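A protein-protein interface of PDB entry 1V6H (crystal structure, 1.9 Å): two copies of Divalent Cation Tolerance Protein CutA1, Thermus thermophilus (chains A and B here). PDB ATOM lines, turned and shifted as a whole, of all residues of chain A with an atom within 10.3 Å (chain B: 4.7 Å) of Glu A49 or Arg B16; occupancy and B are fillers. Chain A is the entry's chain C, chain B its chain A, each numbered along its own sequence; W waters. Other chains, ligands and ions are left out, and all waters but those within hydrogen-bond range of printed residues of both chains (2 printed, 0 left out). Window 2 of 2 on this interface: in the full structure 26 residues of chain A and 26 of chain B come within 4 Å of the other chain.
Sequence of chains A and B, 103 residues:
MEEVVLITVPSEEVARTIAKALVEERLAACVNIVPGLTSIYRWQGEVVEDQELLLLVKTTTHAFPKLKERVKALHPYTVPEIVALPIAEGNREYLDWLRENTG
Among the printed residues, pairs that only touch across the chains: Gly A36 with Ile B33, Leu A37 with Ile B33, Thr A38 with Arg B16, Ile A40 with Ala B19 and Ile A40 with Lys B20.
N of Ile B33 is in hydrogen-bond range of O of Thr A38, at 2.8 Å.
OE1 of Glu A49 lies within salt-bridge range of NH1 of Arg B16.
Printed residues of chain B that touch a printed residue of chain A: Arg B16, Ala B19, Lys B20 and Ile B33.
Hydrophobic or aromatic side chains of chain B within 4 Å of the printed part of chain A: Ala B19 and Ile B33.
Water W2 lies within hydrogen-bond range of the side-chain hydroxyl of Thr A38 (2.7 Å), the backbone carbonyl oxygen of Gly A36 (2.8 Å) and the backbone carbonyl oxygen of Ile B33 (3.5 Å).
Water W1 bridges OG1 of Thr A38 and NH2 of Arg B16.
The backbone carbonyl oxygen (O) of Leu A37 sits close to the side-chain amide oxygen (OE1) of Gln A51.
N of Glu A52 is in hydrogen-bond range of O of Leu A37 (3.0 Å).
OG1 of Thr A38 sits at hydrogen-bond distance from NE2 of Gln A51, at 3.0 Å.
No position is printed for both chains.
Glu A49 touches just one residue of chain B: Arg B16 (2.8 Å).
Of the printed residues of chain A, Arg B16 touches Thr A38 and Glu A49.
No residue of chain A comes within 4 Å of Ala B15.
No residue of chain A comes within 4 Å of Thr B17.
Of the printed residues of chain A, Lys B20 touches Ile A40.
Of the printed residues of chain B, Ile A40 touches Ala B19 (3.7 Å) and Lys B20 (3.5 Å).
Printed residues of chain B within 4 Å of Gly A36: Ile B33.
Val A47 touches none of the printed residues of chain B.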
ATOM      1  N   GLY A  36     -22.666 -19.312   3.266  1.00  0.00           N
ATOM      2  CA  GLY A  36     -21.392 -19.829   3.744  1.00  0.00           C
ATOM      3  C   GLY A  36     -20.075 -19.339   3.183  1.00  0.00           C
ATOM      4  O   GLY A  36     -19.044 -19.967   3.422  1.00  0.00           O
ATOM      5  N   LEU A  37     -20.074 -18.231   2.454  1.00  0.00           N
ATOM      6  CA  LEU A  37     -18.820 -17.735   1.904  1.00  0.00           C
ATOM      7  C   LEU A  37     -17.876 -17.103   2.919  1.00  0.00           C
ATOM      8  O   LEU A  37     -18.306 -16.464   3.878  1.00  0.00           O
ATOM      9  CB  LEU A  37     -19.078 -16.700   0.803  1.00  0.00           C
ATOM     10  CG  LEU A  37     -19.308 -17.169  -0.632  1.00  0.00           C
ATOM     11  CD1 LEU A  37     -20.576 -18.001  -0.725  1.00  0.00           C
ATOM     12  CD2 LEU A  37     -19.410 -15.948  -1.526  1.00  0.00           C
ATOM     13  N   THR A  38     -16.581 -17.314   2.705  1.00  0.00           N
ATOM     14  CA  THR A  38     -15.545 -16.683   3.511  1.00  0.00           C
ATOM     15  C   THR A  38     -14.871 -15.821   2.453  1.00  0.00           C
ATOM     16  O   THR A  38     -14.456 -16.329   1.409  1.00  0.00           O
ATOM     17  CB  THR A  38     -14.512 -17.676   4.061  1.00  0.00           C
ATOM     18  OG1 THR A  38     -15.103 -18.455   5.107  1.00  0.00           O
ATOM     19  CG2 THR A  38     -13.321 -16.926   4.623  1.00  0.00           C
ATOM     20  N   SER A  39     -14.783 -14.520   2.697  1.00  0.00           N
ATOM     21  CA  SER A  39     -14.181 -13.624   1.721  1.00  0.00           C
ATOM     22  C   SER A  39     -12.922 -12.949   2.231  1.00  0.00           C
ATOM     23  O   SER A  39     -12.880 -12.443   3.357  1.00  0.00           O
ATOM     24  CB  SER A  39     -15.199 -12.567   1.293  1.00  0.00           C
ATOM     25  OG  SER A  39     -16.303 -13.174   0.649  1.00  0.00           O
ATOM     26  N   ILE A  40     -11.886 -12.963   1.400  1.00  0.00           N
ATOM     27  CA  ILE A  40     -10.615 -12.337   1.738  1.00  0.00           C
ATOM     28  C   ILE A  40     -10.387 -11.248   0.693  1.00  0.00           C
ATOM     29  O   ILE A  40     -10.359 -11.516  -0.514  1.00  0.00           O
ATOM     30  CB  ILE A  40      -9.471 -13.378   1.725  1.00  0.00           C
ATOM     31  CG1 ILE A  40      -9.713 -14.401   2.839  1.00  0.00           C
ATOM     32  CG2 ILE A  40      -8.132 -12.692   1.913  1.00  0.00           C
ATOM     33  CD1 ILE A  40      -8.710 -15.546   2.873  1.00  0.00           C
ATOM     34  N   TYR A  41     -10.233 -10.014   1.156  1.00  0.00           N
ATOM     35  CA  TYR A  41     -10.073  -8.901   0.235  1.00  0.00           C
ATOM     36  C   TYR A  41      -9.327  -7.703   0.799  1.00  0.00           C
ATOM     37  O   TYR A  41      -8.962  -7.661   1.981  1.00  0.00           O
ATOM     38  CB  TYR A  41     -11.453  -8.428  -0.236  1.00  0.00           C
ATOM     39  CG  TYR A  41     -12.353  -8.036   0.907  1.00  0.00           C
ATOM     40  CD1 TYR A  41     -13.151  -8.982   1.550  1.00  0.00           C
ATOM     41  CD2 TYR A  41     -12.386  -6.720   1.373  1.00  0.00           C
ATOM     42  CE1 TYR A  41     -13.962  -8.628   2.629  1.00  0.00           C
ATOM     43  CE2 TYR A  41     -13.196  -6.356   2.453  1.00  0.00           C
ATOM     44  CZ  TYR A  41     -13.980  -7.312   3.075  1.00  0.00           C
ATOM     45  OH  TYR A  41     -14.787  -6.953   4.132  1.00  0.00           O
ATOM     46  N   ARG A  42      -9.133  -6.721  -0.075  1.00  0.00           N
ATOM     47  CA  ARG A  42      -8.433  -5.487   0.258  1.00  0.00           C
ATOM     48  C   ARG A  42      -9.407  -4.418   0.721  1.00  0.00           C
ATOM     49  O   ARG A  42     -10.439  -4.196   0.094  1.00  0.00           O
ATOM     50  CB  ARG A  42      -7.696  -4.945  -0.971  1.00  0.00           C
ATOM     51  CG  ARG A  42      -6.485  -5.736  -1.408  1.00  0.00           C
ATOM     52  CD  ARG A  42      -5.235  -5.344  -0.619  1.00  0.00           C
ATOM     53  NE  ARG A  42      -4.102  -6.177  -1.010  1.00  0.00           N
ATOM     54  CZ  ARG A  42      -2.915  -6.170  -0.414  1.00  0.00           C
ATOM     55  NH1 ARG A  42      -2.679  -5.362   0.616  1.00  0.00           N
ATOM     56  NH2 ARG A  42      -1.967  -6.994  -0.835  1.00  0.00           N
ATOM     57  N   TRP A  43      -9.072  -3.767   1.826  1.00  0.00           N
ATOM     58  CA  TRP A  43      -9.872  -2.676   2.353  1.00  0.00           C
ATOM     59  C   TRP A  43      -8.876  -1.683   2.928  1.00  0.00           C
ATOM     60  O   TRP A  43      -8.024  -2.053   3.734  1.00  0.00           O
ATOM     61  CB  TRP A  43     -10.820  -3.148   3.454  1.00  0.00           C
ATOM     62  CG  TRP A  43     -11.663  -2.033   3.990  1.00  0.00           C
ATOM     63  CD1 TRP A  43     -12.532  -1.249   3.282  1.00  0.00           C
ATOM     64  CD2 TRP A  43     -11.710  -1.564   5.344  1.00  0.00           C
ATOM     65  NE1 TRP A  43     -13.114  -0.318   4.111  1.00  0.00           N
ATOM     66  CE2 TRP A  43     -12.625  -0.486   5.381  1.00  0.00           C
ATOM     67  CE3 TRP A  43     -11.061  -1.943   6.529  1.00  0.00           C
ATOM     68  CZ2 TRP A  43     -12.916   0.215   6.559  1.00  0.00           C
ATOM     69  CZ3 TRP A  43     -11.349  -1.245   7.705  1.00  0.00           C
ATOM     70  CH2 TRP A  43     -12.268  -0.176   7.707  1.00  0.00           C
ATOM     71  N   GLU A  46      -5.311  -2.749   3.229  1.00  0.00           N
ATOM     72  CA  GLU A  46      -4.954  -3.930   4.012  1.00  0.00           C
ATOM     73  C   GLU A  46      -5.822  -5.150   3.697  1.00  0.00           C
ATOM     74  O   GLU A  46      -6.931  -5.024   3.170  1.00  0.00           O
ATOM     75  CB  GLU A  46      -5.039  -3.602   5.507  1.00  0.00           C
ATOM     76  CG  GLU A  46      -4.067  -2.512   5.947  1.00  0.00           C
ATOM     77  CD  GLU A  46      -2.611  -2.966   5.901  1.00  0.00           C
ATOM     78  OE1 GLU A  46      -2.232  -3.838   6.718  1.00  0.00           O
ATOM     79  OE2 GLU A  46      -1.849  -2.457   5.046  1.00  0.00           O
ATOM     80  N   VAL A  47      -5.312  -6.333   4.035  1.00  0.00           N
ATOM     81  CA  VAL A  47      -6.026  -7.577   3.774  1.00  0.00           C
ATOM     82  C   VAL A  47      -6.923  -8.000   4.932  1.00  0.00           C
ATOM     83  O   VAL A  47      -6.447  -8.280   6.030  1.00  0.00           O
ATOM     84  CB  VAL A  47      -5.039  -8.729   3.470  1.00  0.00           C
ATOM     85  CG1 VAL A  47      -5.804 -10.009   3.182  1.00  0.00           C
ATOM     86  CG2 VAL A  47      -4.164  -8.366   2.291  1.00  0.00           C
ATOM     87  N   VAL A  48      -8.226  -8.058   4.679  1.00  0.00           N
ATOM     88  CA  VAL A  48      -9.168  -8.454   5.715  1.00  0.00           C
ATOM     89  C   VAL A  48      -9.951  -9.696   5.308  1.00  0.00           C
ATOM     90  O   VAL A  48      -9.893 -10.135   4.158  1.00  0.00           O
ATOM     91  CB  VAL A  48     -10.161  -7.315   6.039  1.00  0.00           C
ATOM     92  CG1 VAL A  48      -9.400  -6.071   6.495  1.00  0.00           C
ATOM     93  CG2 VAL A  48     -11.013  -7.004   4.830  1.00  0.00           C
ATOM     94  N   GLU A  49     -10.680 -10.251   6.266  1.00  0.00           N
ATOM     95  CA  GLU A  49     -11.476 -11.453   6.045  1.00  0.00           C
ATOM     96  C   GLU A  49     -12.864 -11.228   6.603  1.00  0.00           C
ATOM     97  O   GLU A  49     -13.011 -10.642   7.673  1.00  0.00           O
ATOM     98  CB  GLU A  49     -10.839 -12.634   6.769  1.00  0.00           C
ATOM     99  CG  GLU A  49     -11.521 -13.953   6.520  1.00  0.00           C
ATOM    100  CD  GLU A  49     -10.970 -15.041   7.414  1.00  0.00           C
ATOM    101  OE1 GLU A  49      -9.743 -15.044   7.651  1.00  0.00           O
ATOM    102  OE2 GLU A  49     -11.757 -15.890   7.868  1.00  0.00           O
ATOM    103  N   ASP A  50     -13.880 -11.705   5.893  1.00  0.00           N
ATOM    104  CA  ASP A  50     -15.247 -11.522   6.351  1.00  0.00           C
ATOM    105  C   ASP A  50     -16.138 -12.672   5.885  1.00  0.00           C
ATOM    106  O   ASP A  50     -15.746 -13.456   5.020  1.00  0.00           O
ATOM    107  CB  ASP A  50     -15.761 -10.178   5.816  1.00  0.00           C
ATOM    108  CG  ASP A  50     -17.035  -9.724   6.490  1.00  0.00           C
ATOM    109  OD1 ASP A  50     -17.282 -10.131   7.642  1.00  0.00           O
ATOM    110  OD2 ASP A  50     -17.784  -8.940   5.866  1.00  0.00           O
ATOM    111  N   GLN A  51     -17.322 -12.790   6.483  1.00  0.00           N
ATOM    112  CA  GLN A  51     -18.282 -13.819   6.102  1.00  0.00           C
ATOM    113  C   GLN A  51     -19.325 -13.164   5.197  1.00  0.00           C
ATOM    114  O   GLN A  51     -19.751 -12.041   5.455  1.00  0.00           O
ATOM    115  CB  GLN A  51     -18.964 -14.416   7.341  1.00  0.00           C
ATOM    116  CG  GLN A  51     -18.053 -15.299   8.177  1.00  0.00           C
ATOM    117  CD  GLN A  51     -17.563 -16.512   7.401  1.00  0.00           C
ATOM    118  OE1 GLN A  51     -18.348 -17.395   7.046  1.00  0.00           O
ATOM    119  NE2 GLN A  51     -16.263 -16.556   7.123  1.00  0.00           N
ATOM    120  N   GLU A  52     -19.723 -13.857   4.134  1.00  0.00           N
ATOM    121  CA  GLU A  52     -20.702 -13.309   3.192  1.00  0.00           C
ATOM    122  C   GLU A  52     -21.561 -14.397   2.557  1.00  0.00           C
ATOM    123  O   GLU A  52     -21.408 -15.582   2.846  1.00  0.00           O
ATOM    124  CB  GLU A  52     -19.993 -12.556   2.052  1.00  0.00           C
ATOM    125  CG  GLU A  52     -19.194 -11.315   2.444  1.00  0.00           C
ATOM    126  CD  GLU A  52     -18.628 -10.594   1.219  1.00  0.00           C
ATOM    127  OE1 GLU A  52     -17.841 -11.207   0.470  1.00  0.00           O
ATOM    128  OE2 GLU A  52     -18.978  -9.416   0.995  1.00  0.00           O
ATOM    129  N   TYR A  77     -22.687  -1.928   1.793  1.00  0.00           N
ATOM    130  CA  TYR A  77     -21.304  -1.600   1.419  1.00  0.00           C
ATOM    131  C   TYR A  77     -21.206  -0.287   0.657  1.00  0.00           C
ATOM    132  O   TYR A  77     -22.096   0.066  -0.116  1.00  0.00           O
ATOM    133  CB  TYR A  77     -20.677  -2.682   0.522  1.00  0.00           C
ATOM    134  CG  TYR A  77     -20.458  -4.048   1.143  1.00  0.00           C
ATOM    135  CD1 TYR A  77     -19.965  -5.103   0.372  1.00  0.00           C
ATOM    136  CD2 TYR A  77     -20.779  -4.303   2.477  1.00  0.00           C
ATOM    137  CE1 TYR A  77     -19.804  -6.383   0.907  1.00  0.00           C
ATOM    138  CE2 TYR A  77     -20.620  -5.581   3.027  1.00  0.00           C
ATOM    139  CZ  TYR A  77     -20.135  -6.614   2.233  1.00  0.00           C
ATOM    140  OH  TYR A  77     -20.005  -7.883   2.753  1.00  0.00           O
ATOM    141  N   GLU B  12     -10.151 -26.838   3.077  1.00  0.00           N
ATOM    142  CA  GLU B  12     -10.263 -25.467   3.543  1.00  0.00           C
ATOM    143  C   GLU B  12      -8.875 -24.881   3.788  1.00  0.00           C
ATOM    144  O   GLU B  12      -8.665 -23.680   3.619  1.00  0.00           O
ATOM    145  CB  GLU B  12     -11.079 -25.419   4.831  1.00  0.00           C
ATOM    146  CG  GLU B  12     -11.203 -24.035   5.426  1.00  0.00           C
ATOM    147  CD  GLU B  12     -11.688 -24.077   6.859  1.00  0.00           C
ATOM    148  OE1 GLU B  12     -12.725 -24.724   7.111  1.00  0.00           O
ATOM    149  OE2 GLU B  12     -11.032 -23.463   7.730  1.00  0.00           O
ATOM    150  N   GLU B  13      -7.926 -25.721   4.198  1.00  0.00           N
ATOM    151  CA  GLU B  13      -6.573 -25.227   4.431  1.00  0.00           C
ATOM    152  C   GLU B  13      -5.972 -24.734   3.119  1.00  0.00           C
ATOM    153  O   GLU B  13      -5.327 -23.684   3.079  1.00  0.00           O
ATOM    154  CB  GLU B  13      -5.686 -26.316   5.048  1.00  0.00           C
ATOM    155  CG  GLU B  13      -6.072 -26.662   6.481  1.00  0.00           C
ATOM    156  CD  GLU B  13      -7.033 -27.833   6.574  1.00  0.00           C
ATOM    157  OE1 GLU B  13      -7.790 -28.072   5.609  1.00  0.00           O
ATOM    158  OE2 GLU B  13      -7.034 -28.515   7.621  1.00  0.00           O
ATOM    159  N   VAL B  14      -6.181 -25.488   2.041  1.00  0.00           N
ATOM    160  CA  VAL B  14      -5.661 -25.069   0.751  1.00  0.00           C
ATOM    161  C   VAL B  14      -6.460 -23.844   0.287  1.00  0.00           C
ATOM    162  O   VAL B  14      -5.882 -22.891  -0.217  1.00  0.00           O
ATOM    163  CB  VAL B  14      -5.747 -26.205  -0.319  1.00  0.00           C
ATOM    164  CG1 VAL B  14      -5.400 -25.648  -1.700  1.00  0.00           C
ATOM    165  CG2 VAL B  14      -4.757 -27.338   0.025  1.00  0.00           C
ATOM    166  N   ALA B  15      -7.778 -23.856   0.485  1.00  0.00           N
ATOM    167  CA  ALA B  15      -8.600 -22.716   0.076  1.00  0.00           C
ATOM    168  C   ALA B  15      -8.100 -21.416   0.716  1.00  0.00           C
ATOM    169  O   ALA B  15      -7.896 -20.419   0.027  1.00  0.00           O
ATOM    170  CB  ALA B  15     -10.068 -22.948   0.445  1.00  0.00           C
ATOM    171  N   ARG B  16      -7.899 -21.437   2.031  1.00  0.00           N
ATOM    172  CA  ARG B  16      -7.434 -20.255   2.754  1.00  0.00           C
ATOM    173  C   ARG B  16      -6.007 -19.824   2.405  1.00  0.00           C
ATOM    174  O   ARG B  16      -5.734 -18.632   2.256  1.00  0.00           O
ATOM    175  CB  ARG B  16      -7.559 -20.487   4.271  1.00  0.00           C
ATOM    176  CG  ARG B  16      -9.004 -20.639   4.760  1.00  0.00           C
ATOM    177  CD  ARG B  16      -9.064 -20.821   6.281  1.00  0.00           C
ATOM    178  NE  ARG B  16      -8.452 -19.690   6.975  1.00  0.00           N
ATOM    179  CZ  ARG B  16      -9.064 -18.533   7.213  1.00  0.00           C
ATOM    180  NH1 ARG B  16      -8.417 -17.557   7.840  1.00  0.00           N
ATOM    181  NH2 ARG B  16     -10.327 -18.362   6.852  1.00  0.00           N
ATOM    182  N   THR B  17      -5.099 -20.781   2.257  1.00  0.00           N
ATOM    183  CA  THR B  17      -3.722 -20.450   1.927  1.00  0.00           C
ATOM    184  C   THR B  17      -3.602 -19.813   0.536  1.00  0.00           C
ATOM    185  O   THR B  17      -2.873 -18.837   0.354  1.00  0.00           O
ATOM    186  CB  THR B  17      -2.824 -21.703   1.992  1.00  0.00           C
ATOM    187  OG1 THR B  17      -2.856 -22.238   3.324  1.00  0.00           O
ATOM    188  CG2 THR B  17      -1.394 -21.358   1.616  1.00  0.00           C
ATOM    189  N   ILE B  18      -4.309 -20.369  -0.446  1.00  0.00           N
ATOM    190  CA  ILE B  18      -4.254 -19.813  -1.788  1.00  0.00           C
ATOM    191  C   ILE B  18      -4.987 -18.468  -1.815  1.00  0.00           C
ATOM    192  O   ILE B  18      -4.496 -17.501  -2.397  1.00  0.00           O
ATOM    193  CB  ILE B  18      -4.871 -20.783  -2.831  1.00  0.00           C
ATOM    194  CG1 ILE B  18      -3.950 -22.002  -3.004  1.00  0.00           C
ATOM    195  CG2 ILE B  18      -5.072 -20.069  -4.173  1.00  0.00           C
ATOM    196  CD1 ILE B  18      -4.466 -23.040  -3.992  1.00  0.00           C
ATOM    197  N   ALA B  19      -6.145 -18.399  -1.165  1.00  0.00           N
ATOM    198  CA  ALA B  19      -6.920 -17.153  -1.148  1.00  0.00           C
ATOM    199  C   ALA B  19      -6.114 -16.006  -0.560  1.00  0.00           C
ATOM    200  O   ALA B  19      -6.085 -14.909  -1.118  1.00  0.00           O
ATOM    201  CB  ALA B  19      -8.224 -17.339  -0.354  1.00  0.00           C
ATOM    202  N   LYS B  20      -5.456 -16.261   0.566  1.00  0.00           N
ATOM    203  CA  LYS B  20      -4.660 -15.235   1.217  1.00  0.00           C
ATOM    204  C   LYS B  20      -3.458 -14.822   0.393  1.00  0.00           C
ATOM    205  O   LYS B  20      -3.149 -13.634   0.286  1.00  0.00           O
ATOM    206  CB  LYS B  20      -4.205 -15.719   2.596  1.00  0.00           C
ATOM    207  CG  LYS B  20      -5.319 -15.726   3.627  1.00  0.00           C
ATOM    208  CD  LYS B  20      -4.872 -16.349   4.938  1.00  0.00           C
ATOM    209  CE  LYS B  20      -4.638 -17.844   4.781  1.00  0.00           C
ATOM    210  NZ  LYS B  20      -4.133 -18.464   6.038  1.00  0.00           N
ATOM    211  N   ILE B  33     -14.523 -17.975  -0.903  1.00  0.00           N
ATOM    212  CA  ILE B  33     -14.370 -19.410  -0.744  1.00  0.00           C
ATOM    213  C   ILE B  33     -15.766 -19.981  -0.518  1.00  0.00           C
ATOM    214  O   ILE B  33     -16.426 -19.639   0.458  1.00  0.00           O
ATOM    215  CB  ILE B  33     -13.490 -19.772   0.482  1.00  0.00           C
ATOM    216  CG1 ILE B  33     -12.089 -19.172   0.336  1.00  0.00           C
ATOM    217  CG2 ILE B  33     -13.390 -21.287   0.610  1.00  0.00           C
ATOM    218  CD1 ILE B  33     -11.185 -19.407   1.548  1.00  0.00           C
HETATM  219  O   HOH W   1     -12.718 -20.172   5.926  1.00  0.00           O
HETATM  220  O   HOH W   2     -16.351 -20.542   3.827  1.00  0.00           O
